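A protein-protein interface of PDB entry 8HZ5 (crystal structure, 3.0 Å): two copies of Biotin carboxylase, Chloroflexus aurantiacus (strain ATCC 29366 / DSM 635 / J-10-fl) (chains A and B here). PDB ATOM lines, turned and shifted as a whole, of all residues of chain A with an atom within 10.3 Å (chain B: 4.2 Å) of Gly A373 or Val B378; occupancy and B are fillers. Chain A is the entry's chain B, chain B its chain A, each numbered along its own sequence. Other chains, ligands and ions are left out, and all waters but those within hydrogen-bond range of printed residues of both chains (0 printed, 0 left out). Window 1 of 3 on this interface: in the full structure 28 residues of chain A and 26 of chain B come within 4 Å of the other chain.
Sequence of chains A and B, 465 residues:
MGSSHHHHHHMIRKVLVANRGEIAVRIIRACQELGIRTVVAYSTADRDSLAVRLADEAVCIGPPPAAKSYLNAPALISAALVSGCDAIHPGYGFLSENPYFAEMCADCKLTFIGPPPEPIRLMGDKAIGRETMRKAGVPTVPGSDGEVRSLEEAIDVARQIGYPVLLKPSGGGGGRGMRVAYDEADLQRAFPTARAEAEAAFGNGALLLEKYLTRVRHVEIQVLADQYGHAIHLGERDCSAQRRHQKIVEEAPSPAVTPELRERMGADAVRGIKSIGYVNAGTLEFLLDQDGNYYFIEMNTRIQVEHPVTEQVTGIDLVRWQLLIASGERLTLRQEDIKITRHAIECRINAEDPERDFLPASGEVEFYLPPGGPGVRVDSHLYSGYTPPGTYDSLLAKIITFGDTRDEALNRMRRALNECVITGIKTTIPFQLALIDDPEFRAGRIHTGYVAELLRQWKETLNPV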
ATOM      1  N   ARG A  29      -1.685  18.955   2.803  1.00  0.00           N
ATOM      2  CA  ARG A  29      -1.771  19.781   3.979  1.00  0.00           C
ATOM      3  C   ARG A  29      -1.082  19.168   5.126  1.00  0.00           C
ATOM      4  O   ARG A  29      -0.396  19.830   5.861  1.00  0.00           O
ATOM      5  CB  ARG A  29      -3.232  20.008   4.306  1.00  0.00           C
ATOM      6  CG  ARG A  29      -3.849  21.157   3.543  1.00  0.00           C
ATOM      7  CD  ARG A  29      -5.363  21.208   3.625  1.00  0.00           C
ATOM      8  NE  ARG A  29      -5.859  22.391   2.931  1.00  0.00           N
ATOM      9  CZ  ARG A  29      -7.107  22.556   2.516  1.00  0.00           C
ATOM     10  NH1 ARG A  29      -8.002  21.603   2.704  1.00  0.00           N
ATOM     11  NH2 ARG A  29      -7.456  23.668   1.892  1.00  0.00           N
ATOM     12  N   GLN A 312     -12.120  15.566  14.965  1.00  0.00           N
ATOM     13  CA  GLN A 312     -12.700  16.717  15.587  1.00  0.00           C
ATOM     14  C   GLN A 312     -13.278  16.419  16.938  1.00  0.00           C
ATOM     15  O   GLN A 312     -13.631  17.334  17.662  1.00  0.00           O
ATOM     16  CB  GLN A 312     -13.747  17.301  14.669  1.00  0.00           C
ATOM     17  CG  GLN A 312     -13.219  17.781  13.339  1.00  0.00           C
ATOM     18  CD  GLN A 312     -12.551  19.127  13.409  1.00  0.00           C
ATOM     19  OE1 GLN A 312     -11.503  19.297  14.016  1.00  0.00           O
ATOM     20  NE2 GLN A 312     -13.146  20.093  12.752  1.00  0.00           N
ATOM     21  N   TYR A 368     -17.476  30.070  -5.568  1.00  0.00           N
ATOM     22  CA  TYR A 368     -17.352  29.195  -4.408  1.00  0.00           C
ATOM     23  C   TYR A 368     -17.008  30.029  -3.172  1.00  0.00           C
ATOM     24  O   TYR A 368     -16.041  30.804  -3.181  1.00  0.00           O
ATOM     25  CB  TYR A 368     -16.305  28.112  -4.625  1.00  0.00           C
ATOM     26  CG  TYR A 368     -16.029  27.297  -3.368  1.00  0.00           C
ATOM     27  CD1 TYR A 368     -17.046  26.576  -2.744  1.00  0.00           C
ATOM     28  CD2 TYR A 368     -14.758  27.264  -2.796  1.00  0.00           C
ATOM     29  CE1 TYR A 368     -16.795  25.837  -1.588  1.00  0.00           C
ATOM     30  CE2 TYR A 368     -14.507  26.532  -1.656  1.00  0.00           C
ATOM     31  CZ  TYR A 368     -15.527  25.821  -1.052  1.00  0.00           C
ATOM     32  OH  TYR A 368     -15.284  25.085   0.089  1.00  0.00           O
ATOM     33  N   LEU A 369     -17.806  29.851  -2.106  1.00  0.00           N
ATOM     34  CA  LEU A 369     -17.631  30.522  -0.827  1.00  0.00           C
ATOM     35  C   LEU A 369     -17.901  29.569   0.331  1.00  0.00           C
ATOM     36  O   LEU A 369     -19.062  29.225   0.628  1.00  0.00           O
ATOM     37  CB  LEU A 369     -18.546  31.741  -0.733  1.00  0.00           C
ATOM     38  CG  LEU A 369     -18.342  32.600   0.505  1.00  0.00           C
ATOM     39  CD1 LEU A 369     -16.871  32.999   0.656  1.00  0.00           C
ATOM     40  CD2 LEU A 369     -19.238  33.806   0.383  1.00  0.00           C
ATOM     41  N   PRO A 370     -16.792  29.093   0.963  1.00  0.00           N
ATOM     42  CA  PRO A 370     -17.092  28.141   2.008  1.00  0.00           C
ATOM     43  C   PRO A 370     -17.568  28.751   3.274  1.00  0.00           C
ATOM     44  O   PRO A 370     -17.333  29.914   3.555  1.00  0.00           O
ATOM     45  CB  PRO A 370     -15.749  27.496   2.262  1.00  0.00           C
ATOM     46  CG  PRO A 370     -14.759  28.507   1.968  1.00  0.00           C
ATOM     47  CD  PRO A 370     -15.313  29.177   0.774  1.00  0.00           C
ATOM     48  N   PRO A 371     -18.248  27.953   4.064  1.00  0.00           N
ATOM     49  CA  PRO A 371     -18.632  28.478   5.343  1.00  0.00           C
ATOM     50  C   PRO A 371     -17.477  28.544   6.292  1.00  0.00           C
ATOM     51  O   PRO A 371     -16.418  27.986   6.067  1.00  0.00           O
ATOM     52  CB  PRO A 371     -19.629  27.475   5.820  1.00  0.00           C
ATOM     53  CG  PRO A 371     -19.306  26.224   5.120  1.00  0.00           C
ATOM     54  CD  PRO A 371     -18.890  26.669   3.775  1.00  0.00           C
ATOM     55  N   GLY A 372     -17.681  29.240   7.381  1.00  0.00           N
ATOM     56  CA  GLY A 372     -16.646  29.361   8.339  1.00  0.00           C
ATOM     57  C   GLY A 372     -17.144  29.820   9.653  1.00  0.00           C
ATOM     58  O   GLY A 372     -18.295  29.655   9.985  1.00  0.00           O
ATOM     59  N   GLY A 373     -16.248  30.385  10.423  1.00  0.00           N
ATOM     60  CA  GLY A 373     -16.620  30.913  11.693  1.00  0.00           C
ATOM     61  C   GLY A 373     -16.305  29.959  12.764  1.00  0.00           C
ATOM     62  O   GLY A 373     -15.463  29.101  12.615  1.00  0.00           O
ATOM     63  N   PRO A 374     -17.006  30.098  13.866  1.00  0.00           N
ATOM     64  CA  PRO A 374     -16.807  29.126  14.915  1.00  0.00           C
ATOM     65  C   PRO A 374     -17.475  27.794  14.648  1.00  0.00           C
ATOM     66  O   PRO A 374     -18.606  27.733  14.198  1.00  0.00           O
ATOM     67  CB  PRO A 374     -17.403  29.813  16.120  1.00  0.00           C
ATOM     68  CG  PRO A 374     -18.457  30.697  15.562  1.00  0.00           C
ATOM     69  CD  PRO A 374     -17.919  31.178  14.256  1.00  0.00           C
ATOM     70  N   GLY A 375     -16.760  26.717  14.912  1.00  0.00           N
ATOM     71  CA  GLY A 375     -17.336  25.402  14.758  1.00  0.00           C
ATOM     72  C   GLY A 375     -17.463  24.801  13.404  1.00  0.00           C
ATOM     73  O   GLY A 375     -18.263  23.920  13.253  1.00  0.00           O
ATOM     74  N   VAL A 376     -16.710  25.276  12.417  1.00  0.00           N
ATOM     75  CA  VAL A 376     -16.807  24.805  11.036  1.00  0.00           C
ATOM     76  C   VAL A 376     -15.439  24.395  10.483  1.00  0.00           C
ATOM     77  O   VAL A 376     -14.461  25.068  10.763  1.00  0.00           O
ATOM     78  CB  VAL A 376     -17.501  25.848  10.116  1.00  0.00           C
ATOM     79  CG1 VAL A 376     -17.627  25.343   8.697  1.00  0.00           C
ATOM     80  CG2 VAL A 376     -18.879  26.210  10.627  1.00  0.00           C
ATOM     81  N   ARG A 377     -15.346  23.269   9.767  1.00  0.00           N
ATOM     82  CA  ARG A 377     -14.116  22.855   9.110  1.00  0.00           C
ATOM     83  C   ARG A 377     -14.582  22.467   7.747  1.00  0.00           C
ATOM     84  O   ARG A 377     -15.553  21.768   7.618  1.00  0.00           O
ATOM     85  CB  ARG A 377     -13.503  21.657   9.791  1.00  0.00           C
ATOM     86  CG  ARG A 377     -12.270  21.096   9.125  1.00  0.00           C
ATOM     87  CD  ARG A 377     -11.913  19.756   9.730  1.00  0.00           C
ATOM     88  NE  ARG A 377     -10.965  19.004   8.931  1.00  0.00           N
ATOM     89  CZ  ARG A 377     -10.298  17.959   9.385  1.00  0.00           C
ATOM     90  NH1 ARG A 377     -10.483  17.561  10.624  1.00  0.00           N
ATOM     91  NH2 ARG A 377      -9.452  17.318   8.606  1.00  0.00           N
ATOM     92  N   VAL A 378     -13.946  22.990   6.715  1.00  0.00           N
ATOM     93  CA  VAL A 378     -14.332  22.682   5.348  1.00  0.00           C
ATOM     94  C   VAL A 378     -13.203  22.037   4.568  1.00  0.00           C
ATOM     95  O   VAL A 378     -12.176  22.645   4.311  1.00  0.00           O
ATOM     96  CB  VAL A 378     -14.842  23.924   4.586  1.00  0.00           C
ATOM     97  CG1 VAL A 378     -15.305  23.549   3.190  1.00  0.00           C
ATOM     98  CG2 VAL A 378     -15.971  24.590   5.334  1.00  0.00           C
ATOM     99  N   ILE A 399     -18.340  19.515   4.668  1.00  0.00           N
ATOM    100  CA  ILE A 399     -18.476  20.451   5.767  1.00  0.00           C
ATOM    101  C   ILE A 399     -18.643  19.685   7.037  1.00  0.00           C
ATOM    102  O   ILE A 399     -19.468  18.821   7.094  1.00  0.00           O
ATOM    103  CB  ILE A 399     -19.678  21.382   5.606  1.00  0.00           C
ATOM    104  CG1 ILE A 399     -19.703  22.036   4.242  1.00  0.00           C
ATOM    105  CG2 ILE A 399     -19.645  22.474   6.654  1.00  0.00           C
ATOM    106  CD1 ILE A 399     -20.821  23.037   4.150  1.00  0.00           C
ATOM    107  N   ILE A 400     -17.842  19.987   8.041  1.00  0.00           N
ATOM    108  CA  ILE A 400     -17.856  19.281   9.300  1.00  0.00           C
ATOM    109  C   ILE A 400     -18.088  20.287  10.414  1.00  0.00           C
ATOM    110  O   ILE A 400     -17.289  21.171  10.599  1.00  0.00           O
ATOM    111  CB  ILE A 400     -16.505  18.532   9.525  1.00  0.00           C
ATOM    112  CG1 ILE A 400     -16.056  17.770   8.279  1.00  0.00           C
ATOM    113  CG2 ILE A 400     -16.582  17.577  10.701  1.00  0.00           C
ATOM    114  CD1 ILE A 400     -14.838  18.326   7.583  1.00  0.00           C
ATOM    115  N   THR A 401     -19.181  20.162  11.158  1.00  0.00           N
ATOM    116  CA  THR A 401     -19.420  21.063  12.288  1.00  0.00           C
ATOM    117  C   THR A 401     -19.403  20.280  13.602  1.00  0.00           C
ATOM    118  O   THR A 401     -19.687  19.073  13.631  1.00  0.00           O
ATOM    119  CB  THR A 401     -20.751  21.889  12.161  1.00  0.00           C
ATOM    120  OG1 THR A 401     -21.899  21.050  12.348  1.00  0.00           O
ATOM    121  CG2 THR A 401     -20.857  22.588  10.803  1.00  0.00           C
ATOM    122  N   PHE A 402     -19.053  20.978  14.692  1.00  0.00           N
ATOM    123  CA  PHE A 402     -18.884  20.367  16.007  1.00  0.00           C
ATOM    124  C   PHE A 402     -19.435  21.278  17.092  1.00  0.00           C
ATOM    125  O   PHE A 402     -19.563  22.494  16.920  1.00  0.00           O
ATOM    126  CB  PHE A 402     -17.431  20.073  16.328  1.00  0.00           C
ATOM    127  CG  PHE A 402     -16.492  21.157  15.896  1.00  0.00           C
ATOM    128  CD1 PHE A 402     -15.930  21.128  14.614  1.00  0.00           C
ATOM    129  CD2 PHE A 402     -16.116  22.160  16.781  1.00  0.00           C
ATOM    130  CE1 PHE A 402     -15.058  22.102  14.200  1.00  0.00           C
ATOM    131  CE2 PHE A 402     -15.228  23.126  16.387  1.00  0.00           C
ATOM    132  CZ  PHE A 402     -14.689  23.099  15.085  1.00  0.00           C
ATOM    133  N   ARG A 412     -24.995  24.488  14.000  1.00  0.00           N
ATOM    134  CA  ARG A 412     -23.909  25.140  13.295  1.00  0.00           C
ATOM    135  C   ARG A 412     -23.751  24.717  11.803  1.00  0.00           C
ATOM    136  O   ARG A 412     -23.243  25.395  10.934  1.00  0.00           O
ATOM    137  CB  ARG A 412     -22.623  24.780  13.996  1.00  0.00           C
ATOM    138  CG  ARG A 412     -22.442  25.251  15.412  1.00  0.00           C
ATOM    139  CD  ARG A 412     -21.069  24.860  15.921  1.00  0.00           C
ATOM    140  NE  ARG A 412     -20.869  25.281  17.299  1.00  0.00           N
ATOM    141  CZ  ARG A 412     -20.491  26.495  17.670  1.00  0.00           C
ATOM    142  NH1 ARG A 412     -20.270  27.428  16.768  1.00  0.00           N
ATOM    143  NH2 ARG A 412     -20.342  26.774  18.951  1.00  0.00           N
ATOM    144  N   ARG A 415     -26.226  26.529   9.510  1.00  0.00           N
ATOM    145  CA  ARG A 415     -25.683  27.798   9.177  1.00  0.00           C
ATOM    146  C   ARG A 415     -24.676  27.600   8.126  1.00  0.00           C
ATOM    147  O   ARG A 415     -24.712  28.263   7.124  1.00  0.00           O
ATOM    148  CB  ARG A 415     -25.027  28.361  10.409  1.00  0.00           C
ATOM    149  CG  ARG A 415     -24.258  29.611  10.135  1.00  0.00           C
ATOM    150  CD  ARG A 415     -23.751  30.205  11.407  1.00  0.00           C
ATOM    151  NE  ARG A 415     -22.633  29.507  12.031  1.00  0.00           N
ATOM    152  CZ  ARG A 415     -21.397  29.429  11.554  1.00  0.00           C
ATOM    153  NH1 ARG A 415     -21.072  29.953  10.390  1.00  0.00           N
ATOM    154  NH2 ARG A 415     -20.479  28.800  12.255  1.00  0.00           N
ATOM    155  N   ALA A 416     -23.779  26.658   8.327  1.00  0.00           N
ATOM    156  CA  ALA A 416     -22.743  26.374   7.378  1.00  0.00           C
ATOM    157  C   ALA A 416     -23.265  26.043   6.026  1.00  0.00           C
ATOM    158  O   ALA A 416     -22.727  26.457   5.027  1.00  0.00           O
ATOM    159  CB  ALA A 416     -21.956  25.227   7.890  1.00  0.00           C
ATOM    160  N   GLU A 419     -24.693  29.007   4.215  1.00  0.00           N
ATOM    161  CA  GLU A 419     -23.616  29.909   3.883  1.00  0.00           C
ATOM    162  C   GLU A 419     -22.790  29.426   2.700  1.00  0.00           C
ATOM    163  O   GLU A 419     -22.133  30.212   2.063  1.00  0.00           O
ATOM    164  CB  GLU A 419     -22.703  30.087   5.090  1.00  0.00           C
ATOM    165  CG  GLU A 419     -23.254  30.931   6.207  1.00  0.00           C
ATOM    166  CD  GLU A 419     -22.234  31.167   7.284  1.00  0.00           C
ATOM    167  OE1 GLU A 419     -21.110  30.663   7.158  1.00  0.00           O
ATOM    168  OE2 GLU A 419     -22.559  31.860   8.256  1.00  0.00           O
ATOM    169  N   ARG B  29     -23.619  34.902  12.748  1.00  0.00           N
ATOM    170  CA  ARG B  29     -23.414  33.471  12.958  1.00  0.00           C
ATOM    171  C   ARG B  29     -23.843  33.035  14.357  1.00  0.00           C
ATOM    172  O   ARG B  29     -24.539  32.026  14.513  1.00  0.00           O
ATOM    173  CB  ARG B  29     -21.952  33.130  12.697  1.00  0.00           C
ATOM    174  CG  ARG B  29     -21.609  33.300  11.247  1.00  0.00           C
ATOM    175  CD  ARG B  29     -20.147  33.177  10.964  1.00  0.00           C
ATOM    176  NE  ARG B  29     -19.989  32.921   9.540  1.00  0.00           N
ATOM    177  CZ  ARG B  29     -18.846  33.009   8.876  1.00  0.00           C
ATOM    178  NH1 ARG B  29     -17.714  33.335   9.492  1.00  0.00           N
ATOM    179  NH2 ARG B  29     -18.840  32.738   7.568  1.00  0.00           N
ATOM    180  N   TYR B 368     -11.080  34.786  -3.860  1.00  0.00           N
ATOM    181  CA  TYR B 368     -10.858  34.538  -2.461  1.00  0.00           C
ATOM    182  C   TYR B 368     -11.008  33.094  -2.202  1.00  0.00           C
ATOM    183  O   TYR B 368     -12.081  32.539  -2.368  1.00  0.00           O
ATOM    184  CB  TYR B 368     -11.830  35.294  -1.583  1.00  0.00           C
ATOM    185  CG  TYR B 368     -11.707  35.035  -0.114  1.00  0.00           C
ATOM    186  CD1 TYR B 368     -10.491  35.122   0.529  1.00  0.00           C
ATOM    187  CD2 TYR B 368     -12.817  34.714   0.631  1.00  0.00           C
ATOM    188  CE1 TYR B 368     -10.384  34.881   1.877  1.00  0.00           C
ATOM    189  CE2 TYR B 368     -12.722  34.488   1.980  1.00  0.00           C
ATOM    190  CZ  TYR B 368     -11.502  34.569   2.593  1.00  0.00           C
ATOM    191  OH  TYR B 368     -11.408  34.331   3.931  1.00  0.00           O
ATOM    192  N   PRO B 371      -8.348  29.561   3.585  1.00  0.00           N
ATOM    193  CA  PRO B 371      -7.689  28.301   3.801  1.00  0.00           C
ATOM    194  C   PRO B 371      -8.683  27.308   4.399  1.00  0.00           C
ATOM    195  O   PRO B 371      -9.875  27.553   4.470  1.00  0.00           O
ATOM    196  CB  PRO B 371      -6.608  28.661   4.780  1.00  0.00           C
ATOM    197  CG  PRO B 371      -7.040  29.907   5.445  1.00  0.00           C
ATOM    198  CD  PRO B 371      -7.804  30.643   4.416  1.00  0.00           C
ATOM    199  N   VAL B 376      -7.745  25.040  11.318  1.00  0.00           N
ATOM    200  CA  VAL B 376      -7.880  26.376  10.773  1.00  0.00           C
ATOM    201  C   VAL B 376      -9.261  26.941  10.995  1.00  0.00           C
ATOM    202  O   VAL B 376     -10.239  26.227  10.870  1.00  0.00           O
ATOM    203  CB  VAL B 376      -7.595  26.403   9.251  1.00  0.00           C
ATOM    204  CG1 VAL B 376      -7.423  27.815   8.735  1.00  0.00           C
ATOM    205  CG2 VAL B 376      -6.368  25.594   8.895  1.00  0.00           C
ATOM    206  N   ARG B 377      -9.347  28.220  11.348  1.00  0.00           N
ATOM    207  CA  ARG B 377     -10.617  28.888  11.492  1.00  0.00           C
ATOM    208  C   ARG B 377     -10.455  30.174  10.783  1.00  0.00           C
ATOM    209  O   ARG B 377      -9.514  30.896  11.005  1.00  0.00           O
ATOM    210  CB  ARG B 377     -10.946  29.140  12.940  1.00  0.00           C
ATOM    211  CG  ARG B 377     -12.276  29.801  13.182  1.00  0.00           C
ATOM    212  CD  ARG B 377     -12.378  30.201  14.629  1.00  0.00           C
ATOM    213  NE  ARG B 377     -13.295  31.301  14.841  1.00  0.00           N
ATOM    214  CZ  ARG B 377     -13.983  31.474  15.955  1.00  0.00           C
ATOM    215  NH1 ARG B 377     -13.848  30.616  16.946  1.00  0.00           N
ATOM    216  NH2 ARG B 377     -14.795  32.501  16.079  1.00  0.00           N
ATOM    217  N   VAL B 378     -11.364  30.444   9.878  1.00  0.00           N
ATOM    218  CA  VAL B 378     -11.321  31.678   9.146  1.00  0.00           C
ATOM    219  C   VAL B 378     -12.518  32.515   9.469  1.00  0.00           C
ATOM    220  O   VAL B 378     -13.640  32.110   9.246  1.00  0.00           O
ATOM    221  CB  VAL B 378     -11.244  31.469   7.630  1.00  0.00           C
ATOM    222  CG1 VAL B 378     -10.753  32.725   6.938  1.00  0.00           C
ATOM    223  CG2 VAL B 378     -10.380  30.273   7.282  1.00  0.00           C
ATOM    224  N   ASP B 379     -12.275  33.685  10.020  1.00  0.00           N
ATOM    225  CA  ASP B 379     -13.330  34.600  10.333  1.00  0.00           C
ATOM    226  C   ASP B 379     -13.169  35.776   9.405  1.00  0.00           C
ATOM    227  O   ASP B 379     -12.280  36.578   9.583  1.00  0.00           O
ATOM    228  CB  ASP B 379     -13.217  35.005  11.796  1.00  0.00           C
ATOM    229  CG  ASP B 379     -13.891  34.045  12.731  1.00  0.00           C
ATOM    230  OD1 ASP B 379     -13.737  32.836  12.538  1.00  0.00           O
ATOM    231  OD2 ASP B 379     -14.560  34.499  13.670  1.00  0.00           O
ATOM    232  N   SER B 380     -14.001  35.870   8.386  1.00  0.00           N
ATOM    233  CA  SER B 380     -13.879  36.928   7.404  1.00  0.00           C
ATOM    234  C   SER B 380     -15.184  37.261   6.737  1.00  0.00           C
ATOM    235  O   SER B 380     -16.125  36.500   6.813  1.00  0.00           O
ATOM    236  CB  SER B 380     -12.890  36.512   6.339  1.00  0.00           C
ATOM    237  OG  SER B 380     -12.713  37.500   5.359  1.00  0.00           O
ATOM    238  N   LYS B 398      -9.285  36.979   9.178  1.00  0.00           N
ATOM    239  CA  LYS B 398      -8.602  36.553  10.390  1.00  0.00           C
ATOM    240  C   LYS B 398      -8.468  35.059  10.454  1.00  0.00           C
ATOM    241  O   LYS B 398      -9.422  34.373  10.718  1.00  0.00           O
ATOM    242  CB  LYS B 398      -9.342  37.026  11.625  1.00  0.00           C
ATOM    243  CG  LYS B 398      -8.976  38.421  12.077  1.00  0.00           C
ATOM    244  CD  LYS B 398     -10.112  39.009  12.876  1.00  0.00           C
ATOM    245  CE  LYS B 398     -10.879  37.914  13.578  1.00  0.00           C
ATOM    246  NZ  LYS B 398     -11.742  38.484  14.641  1.00  0.00           N
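Val B378 touches just one residue of chain A: Gly A373 (3.3 Å).
Pro B371 touches none of the printed residues of chain A.
Asp B379 touches one residue of chain A.
Ser B380 touches none of the printed residues of chain A.
Of the printed residues of chain B, Arg A415 touches Arg B29.
Of the printed residues of chain B, Glu A419 touches Arg B29.
Printed residues of chain B within 4 Å of Pro A374: Arg B377 (3.7 Å).
Printed residues of chain B within 4 Å of Gly A372: Arg B29 (3.6 Å).
Leu A369 touches none of the printed residues of chain B.
Pro A371 touches none of the printed residues of chain B.
The nearest printed residue of chain B that does not touch Gly A373 is Val B376 (6.2 Å).
The nearest residue of chain A that does not touch Val B378 is Gly A372 (4.2 Å).
The nearest printed residue of chain B that does not touch Glu A419 is Ser B380 (7.7 Å).
NH1 of Arg A415 sits at hydrogen-bond distance from O of Gly A372, 2.8 Å away.
The backbone NH (N) of Asp B379 lies within hydrogen-bond range of the backbone carbonyl oxygen (O) of Lys B398.
The guanidinium group (NH2) of Arg A415 sits at hydrogen-bond distance from the backbone carbonyl oxygen (O) of Pro A374.
NH1 of Arg A415 is in salt-bridge range of OE2 of Glu A419 (3.2 Å).
The guanidinium group (NE) of Arg B377 lies within salt-bridge range of the side-chain carboxylate (OD1) of Asp B379 (2.8 Å).
The backbone carbonyl oxygen of Pro A374 is in hydrogen-bond range of the guanidinium group of Arg A412.
Positions printed for both chains: 29, 368, 371, 376, 377 and 378.
Among the printed residues, merely in contact across the chains: Gly A373 with Arg B377, Gly A372 with Arg B29, Gly A373 with Asp B379 and Pro A374 with Arg B377.
The backbone NH (N) of Gly A373 sits close to the guanidinium group (NH1) of Arg B29, 3.4 Å away.
OE2 of Glu A419 is in salt-bridge range of NE of Arg B29 (3.1 Å).
The guanidinium group of Arg B29 sits close to the guanidinium group of Arg A415 (3.3 Å).
The backbone carbonyl oxygen of Val B378 is in hydrogen-bond range of the backbone NH of Gly A373.
Of the 21 printed residues of chain A, 5 touch a printed residue of chain B.
Printed residues of chain A that touch a printed residue of chain B: Gly A372, Gly A373, Pro A374, Arg A415 and Glu A419.
Hydrophobic or aromatic side chains of chain A within 4 Å of the printed part of chain B: Pro A374.
Along chain A the printed residues that touch a printed residue of chain B span positions 372 to 419.
Among the printed residues, 8 pairs touch across the chains.
Among the printed residues, Asp or Glu carboxylates within 4 Å of a Lys or Arg side-chain nitrogen of the other chain: Glu A419 with Arg B29.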
